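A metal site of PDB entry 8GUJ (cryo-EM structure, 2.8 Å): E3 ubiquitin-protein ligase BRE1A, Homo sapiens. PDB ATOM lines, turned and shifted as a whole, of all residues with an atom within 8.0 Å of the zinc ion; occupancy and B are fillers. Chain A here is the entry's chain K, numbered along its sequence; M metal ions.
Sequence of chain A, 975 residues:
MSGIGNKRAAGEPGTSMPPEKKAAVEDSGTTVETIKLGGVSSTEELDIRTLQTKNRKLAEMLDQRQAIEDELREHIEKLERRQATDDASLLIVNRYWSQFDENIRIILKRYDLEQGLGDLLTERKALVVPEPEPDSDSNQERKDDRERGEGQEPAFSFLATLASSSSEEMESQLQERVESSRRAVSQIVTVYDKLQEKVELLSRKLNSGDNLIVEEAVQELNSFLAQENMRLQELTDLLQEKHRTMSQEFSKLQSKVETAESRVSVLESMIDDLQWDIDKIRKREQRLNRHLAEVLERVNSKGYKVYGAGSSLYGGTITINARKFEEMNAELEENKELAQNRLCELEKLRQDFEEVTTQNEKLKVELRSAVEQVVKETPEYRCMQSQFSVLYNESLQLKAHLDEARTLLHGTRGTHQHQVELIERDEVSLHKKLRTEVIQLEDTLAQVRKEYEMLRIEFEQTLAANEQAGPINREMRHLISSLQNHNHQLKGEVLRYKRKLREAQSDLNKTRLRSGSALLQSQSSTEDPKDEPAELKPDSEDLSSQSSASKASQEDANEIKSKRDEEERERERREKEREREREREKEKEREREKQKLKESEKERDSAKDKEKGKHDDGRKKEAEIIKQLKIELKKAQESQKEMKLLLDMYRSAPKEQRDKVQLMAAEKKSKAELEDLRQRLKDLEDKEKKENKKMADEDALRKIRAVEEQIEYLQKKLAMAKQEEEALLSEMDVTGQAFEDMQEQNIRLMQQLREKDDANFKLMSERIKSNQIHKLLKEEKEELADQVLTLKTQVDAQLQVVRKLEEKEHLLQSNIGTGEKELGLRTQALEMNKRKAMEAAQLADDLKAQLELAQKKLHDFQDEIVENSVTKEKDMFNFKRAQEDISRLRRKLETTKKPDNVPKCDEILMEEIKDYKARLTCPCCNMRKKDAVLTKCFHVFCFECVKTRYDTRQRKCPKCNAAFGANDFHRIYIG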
ATOM      1  N   LEU A 934      -3.022  -3.332 -15.509  1.00  0.00           N
ATOM      2  CA  LEU A 934      -3.140  -2.516 -14.309  1.00  0.00           C
ATOM      3  C   LEU A 934      -4.374  -1.627 -14.456  1.00  0.00           C
ATOM      4  O   LEU A 934      -4.429  -0.792 -15.371  1.00  0.00           O
ATOM      5  CB  LEU A 934      -1.888  -1.668 -14.095  1.00  0.00           C
ATOM      6  CG  LEU A 934      -0.524  -2.354 -14.181  1.00  0.00           C
ATOM      7  CD1 LEU A 934       0.585  -1.361 -13.860  1.00  0.00           C
ATOM      8  CD2 LEU A 934      -0.457  -3.553 -13.254  1.00  0.00           C
ATOM      9  N   THR A 935      -5.353  -1.811 -13.577  1.00  0.00           N
ATOM     10  CA  THR A 935      -6.651  -1.172 -13.793  1.00  0.00           C
ATOM     11  C   THR A 935      -6.685   0.263 -13.264  1.00  0.00           C
ATOM     12  O   THR A 935      -7.607   1.020 -13.591  1.00  0.00           O
ATOM     13  CB  THR A 935      -7.759  -2.012 -13.155  1.00  0.00           C
ATOM     14  OG1 THR A 935      -7.419  -2.312 -11.806  1.00  0.00           O
ATOM     15  CG2 THR A 935      -7.954  -3.309 -13.920  1.00  0.00           C
ATOM     16  N   LYS A 936      -5.714   0.646 -12.433  1.00  0.00           N
ATOM     17  CA  LYS A 936      -5.621   2.049 -12.025  1.00  0.00           C
ATOM     18  C   LYS A 936      -5.129   2.924 -13.167  1.00  0.00           C
ATOM     19  O   LYS A 936      -5.720   3.958 -13.481  1.00  0.00           O
ATOM     20  CB  LYS A 936      -4.723   2.191 -10.802  1.00  0.00           C
ATOM     21  CG  LYS A 936      -5.451   2.712  -9.565  1.00  0.00           C
ATOM     22  CD  LYS A 936      -6.543   1.766  -9.088  1.00  0.00           C
ATOM     23  CE  LYS A 936      -7.225   2.313  -7.849  1.00  0.00           C
ATOM     24  NZ  LYS A 936      -8.439   1.529  -7.482  1.00  0.00           N
ATOM     25  N   CYS A 937      -4.035   2.520 -13.823  1.00  0.00           N
ATOM     26  CA  CYS A 937      -3.466   3.321 -14.891  1.00  0.00           C
ATOM     27  C   CYS A 937      -3.947   2.914 -16.272  1.00  0.00           C
ATOM     28  O   CYS A 937      -3.537   3.537 -17.260  1.00  0.00           O
ATOM     29  CB  CYS A 937      -1.932   3.261 -14.841  1.00  0.00           C
ATOM     30  SG  CYS A 937      -1.214   1.644 -15.164  1.00  0.00           S
ATOM     31  N   PHE A 938      -4.808   1.891 -16.365  1.00  0.00           N
ATOM     32  CA  PHE A 938      -5.369   1.426 -17.639  1.00  0.00           C
ATOM     33  C   PHE A 938      -4.290   1.054 -18.642  1.00  0.00           C
ATOM     34  O   PHE A 938      -4.376   1.361 -19.835  1.00  0.00           O
ATOM     35  CB  PHE A 938      -6.321   2.473 -18.229  1.00  0.00           C
ATOM     36  CG  PHE A 938      -7.718   2.428 -17.664  1.00  0.00           C
ATOM     37  CD1 PHE A 938      -8.039   1.534 -16.647  1.00  0.00           C
ATOM     38  CD2 PHE A 938      -8.702   3.285 -18.133  1.00  0.00           C
ATOM     39  CE1 PHE A 938      -9.316   1.495 -16.124  1.00  0.00           C
ATOM     40  CE2 PHE A 938      -9.980   3.247 -17.610  1.00  0.00           C
ATOM     41  CZ  PHE A 938     -10.287   2.353 -16.598  1.00  0.00           C
ATOM     42  N   HIS A 939      -3.250   0.383 -18.153  1.00  0.00           N
ATOM     43  CA  HIS A 939      -2.127  -0.041 -18.975  1.00  0.00           C
ATOM     44  C   HIS A 939      -1.960  -1.549 -18.909  1.00  0.00           C
ATOM     45  O   HIS A 939      -2.460  -2.225 -17.997  1.00  0.00           O
ATOM     46  CB  HIS A 939      -0.828   0.653 -18.541  1.00  0.00           C
ATOM     47  CG  HIS A 939      -0.903   2.141 -18.577  1.00  0.00           C
ATOM     48  ND1 HIS A 939      -0.298   2.949 -17.636  1.00  0.00           N
ATOM     49  CD2 HIS A 939      -1.501   2.982 -19.459  1.00  0.00           C
ATOM     50  CE1 HIS A 939      -0.526   4.214 -17.923  1.00  0.00           C
ATOM     51  NE2 HIS A 939      -1.258   4.264 -19.033  1.00  0.00           N
ATOM     52  N   VAL A 940      -1.240  -2.084 -19.899  1.00  0.00           N
ATOM     53  CA  VAL A 940      -1.069  -3.518 -20.076  1.00  0.00           C
ATOM     54  C   VAL A 940       0.416  -3.840 -20.011  1.00  0.00           C
ATOM     55  O   VAL A 940       1.216  -3.231 -20.725  1.00  0.00           O
ATOM     56  CB  VAL A 940      -1.672  -3.985 -21.414  1.00  0.00           C
ATOM     57  CG1 VAL A 940      -1.391  -5.460 -21.648  1.00  0.00           C
ATOM     58  CG2 VAL A 940      -3.159  -3.716 -21.441  1.00  0.00           C
ATOM     59  N   PHE A 941       0.774  -4.780 -19.130  1.00  0.00           N
ATOM     60  CA  PHE A 941       2.120  -5.345 -19.036  1.00  0.00           C
ATOM     61  C   PHE A 941       2.045  -6.858 -19.227  1.00  0.00           C
ATOM     62  O   PHE A 941       0.996  -7.390 -19.588  1.00  0.00           O
ATOM     63  CB  PHE A 941       2.777  -5.044 -17.678  1.00  0.00           C
ATOM     64  CG  PHE A 941       3.318  -3.643 -17.540  1.00  0.00           C
ATOM     65  CD1 PHE A 941       4.137  -3.328 -16.466  1.00  0.00           C
ATOM     66  CD2 PHE A 941       3.052  -2.655 -18.467  1.00  0.00           C
ATOM     67  CE1 PHE A 941       4.655  -2.060 -16.317  1.00  0.00           C
ATOM     68  CE2 PHE A 941       3.566  -1.383 -18.326  1.00  0.00           C
ATOM     69  CZ  PHE A 941       4.364  -1.089 -17.251  1.00  0.00           C
ATOM     70  N   ARG A 949       8.166  -7.778 -10.042  1.00  0.00           N
ATOM     71  CA  ARG A 949       8.337  -6.395  -9.620  1.00  0.00           C
ATOM     72  C   ARG A 949       7.362  -6.054  -8.489  1.00  0.00           C
ATOM     73  O   ARG A 949       7.553  -5.065  -7.774  1.00  0.00           O
ATOM     74  CB  ARG A 949       8.161  -5.477 -10.834  1.00  0.00           C
ATOM     75  CG  ARG A 949       8.570  -4.014 -10.667  1.00  0.00           C
ATOM     76  CD  ARG A 949       7.432  -3.134 -10.221  1.00  0.00           C
ATOM     77  NE  ARG A 949       6.336  -3.127 -11.178  1.00  0.00           N
ATOM     78  CZ  ARG A 949       5.128  -2.690 -10.906  1.00  0.00           C
ATOM     79  NH1 ARG A 949       4.827  -2.186  -9.722  1.00  0.00           N
ATOM     80  NH2 ARG A 949       4.185  -2.750 -11.845  1.00  0.00           N
ATOM     81  N   LYS A 956       4.400   0.432  -7.702  1.00  0.00           N
ATOM     82  CA  LYS A 956       4.206   1.591  -8.574  1.00  0.00           C
ATOM     83  C   LYS A 956       4.388   1.156 -10.017  1.00  0.00           C
ATOM     84  O   LYS A 956       5.201   0.279 -10.322  1.00  0.00           O
ATOM     85  CB  LYS A 956       5.193   2.721  -8.243  1.00  0.00           C
ATOM     86  CG  LYS A 956       5.063   3.272  -6.833  1.00  0.00           C
ATOM     87  CD  LYS A 956       3.689   3.887  -6.607  1.00  0.00           C
ATOM     88  CE  LYS A 956       3.492   5.135  -7.451  1.00  0.00           C
ATOM     89  NZ  LYS A 956       4.428   6.219  -7.068  1.00  0.00           N
ATOM     90  N   CYS A 957       3.630   1.789 -10.917  1.00  0.00           N
ATOM     91  CA  CYS A 957       3.761   1.476 -12.330  1.00  0.00           C
ATOM     92  C   CYS A 957       5.087   2.018 -12.844  1.00  0.00           C
ATOM     93  O   CYS A 957       5.415   3.182 -12.580  1.00  0.00           O
ATOM     94  CB  CYS A 957       2.599   2.048 -13.137  1.00  0.00           C
ATOM     95  SG  CYS A 957       2.612   1.534 -14.880  1.00  0.00           S
ATOM     96  N   PRO A 958       5.883   1.217 -13.547  1.00  0.00           N
ATOM     97  CA  PRO A 958       7.192   1.706 -14.018  1.00  0.00           C
ATOM     98  C   PRO A 958       7.123   2.907 -14.931  1.00  0.00           C
ATOM     99  O   PRO A 958       8.068   3.717 -14.935  1.00  0.00           O
ATOM    100  CB  PRO A 958       7.765   0.476 -14.745  1.00  0.00           C
ATOM    101  CG  PRO A 958       7.152  -0.687 -14.042  1.00  0.00           C
ATOM    102  CD  PRO A 958       5.777  -0.249 -13.620  1.00  0.00           C
ATOM    103  N   LYS A 959       6.059   3.072 -15.714  1.00  0.00           N
ATOM    104  CA  LYS A 959       6.032   4.116 -16.740  1.00  0.00           C
ATOM    105  C   LYS A 959       5.140   5.300 -16.382  1.00  0.00           C
ATOM    106  O   LYS A 959       5.480   6.434 -16.720  1.00  0.00           O
ATOM    107  CB  LYS A 959       5.624   3.524 -18.094  1.00  0.00           C
ATOM    108  CG  LYS A 959       4.186   3.062 -18.217  1.00  0.00           C
ATOM    109  CD  LYS A 959       3.962   2.413 -19.587  1.00  0.00           C
ATOM    110  CE  LYS A 959       2.507   2.050 -19.801  1.00  0.00           C
ATOM    111  NZ  LYS A 959       1.673   3.259 -20.019  1.00  0.00           N
ATOM    112  N   CYS A 960       4.021   5.079 -15.705  1.00  0.00           N
ATOM    113  CA  CYS A 960       3.135   6.186 -15.348  1.00  0.00           C
ATOM    114  C   CYS A 960       3.101   6.461 -13.843  1.00  0.00           C
ATOM    115  O   CYS A 960       2.415   7.398 -13.430  1.00  0.00           O
ATOM    116  CB  CYS A 960       1.713   5.924 -15.843  1.00  0.00           C
ATOM    117  SG  CYS A 960       0.786   4.714 -14.894  1.00  0.00           S
ATOM    118  N   ASN A 961       3.821   5.666 -13.045  1.00  0.00           N
ATOM    119  CA  ASN A 961       3.929   5.882 -11.597  1.00  0.00           C
ATOM    120  C   ASN A 961       2.571   5.844 -10.904  1.00  0.00           C
ATOM    121  O   ASN A 961       2.195   6.777 -10.187  1.00  0.00           O
ATOM    122  CB  ASN A 961       4.672   7.184 -11.277  1.00  0.00           C
ATOM    123  CG  ASN A 961       6.173   6.989 -11.152  1.00  0.00           C
ATOM    124  OD1 ASN A 961       6.752   6.110 -11.799  1.00  0.00           O
ATOM    125  ND2 ASN A 961       6.810   7.804 -10.331  1.00  0.00           N
ATOM    126  N   ALA A 962       1.823   4.776 -11.119  1.00  0.00           N
ATOM    127  CA  ALA A 962       0.517   4.585 -10.495  1.00  0.00           C
ATOM    128  C   ALA A 962       0.598   3.502  -9.441  1.00  0.00           C
ATOM    129  O   ALA A 962       1.078   2.393  -9.702  1.00  0.00           O
ATOM    130  CB  ALA A 962      -0.537   4.236 -11.546  1.00  0.00           C
ATOM    131  N   ALA A 963       0.129   3.821  -8.235  1.00  0.00           N
ATOM    132  CA  ALA A 963       0.123   2.854  -7.148  1.00  0.00           C
ATOM    133  C   ALA A 963      -1.064   1.901  -7.284  1.00  0.00           C
ATOM    134  O   ALA A 963      -2.181   2.329  -7.605  1.00  0.00           O
ATOM    135  CB  ALA A 963       0.064   3.573  -5.793  1.00  0.00           C
ATOM    136  N   PHE A 964      -0.819   0.617  -7.049  1.00  0.00           N
ATOM    137  CA  PHE A 964      -1.860  -0.397  -7.161  1.00  0.00           C
ATOM    138  C   PHE A 964      -1.671  -1.459  -6.089  1.00  0.00           C
ATOM    139  O   PHE A 964      -0.567  -1.657  -5.576  1.00  0.00           O
ATOM    140  CB  PHE A 964      -1.868  -1.050  -8.551  1.00  0.00           C
ATOM    141  CG  PHE A 964      -0.585  -1.720  -8.926  1.00  0.00           C
ATOM    142  CD1 PHE A 964      -0.361  -3.051  -8.607  1.00  0.00           C
ATOM    143  CD2 PHE A 964       0.408  -1.020  -9.607  1.00  0.00           C
ATOM    144  CE1 PHE A 964       0.825  -3.666  -8.946  1.00  0.00           C
ATOM    145  CE2 PHE A 964       1.586  -1.642  -9.946  1.00  0.00           C
ATOM    146  CZ  PHE A 964       1.791  -2.968  -9.616  1.00  0.00           C
HETATM  147 ZN    ZN M   1       0.793   2.602 -15.863  1.00  0.00          ZN
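The backbone carbonyl oxygen (O) of His 939 lies within hydrogen-bond range of the backbone NH (N) of Leu 934, 2.8 Å away.
NE2 of His 939 sits close to NZ of Lys 959.
O of Cys 957 sits close to OD1 of Asn 961, 3.3 Å away.
N of Cys 957 sits at hydrogen-bond distance from O of Ala 962 (2.9 Å).
Of the 18 residues printed, 4 come within 4 Å of the zinc ion.
The nearest printed residue that does not touch the zinc ion is Lys 959 (4.2 Å).
The zinc ion is bound by ND1 of His 939 (2.1 Å), SG of Cys 960 (2.3 Å), SG of Cys 957 (2.3 Å) and SG of Cys 937 (2.3 Å).
The zinc ion has four donor atoms within binding distance.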
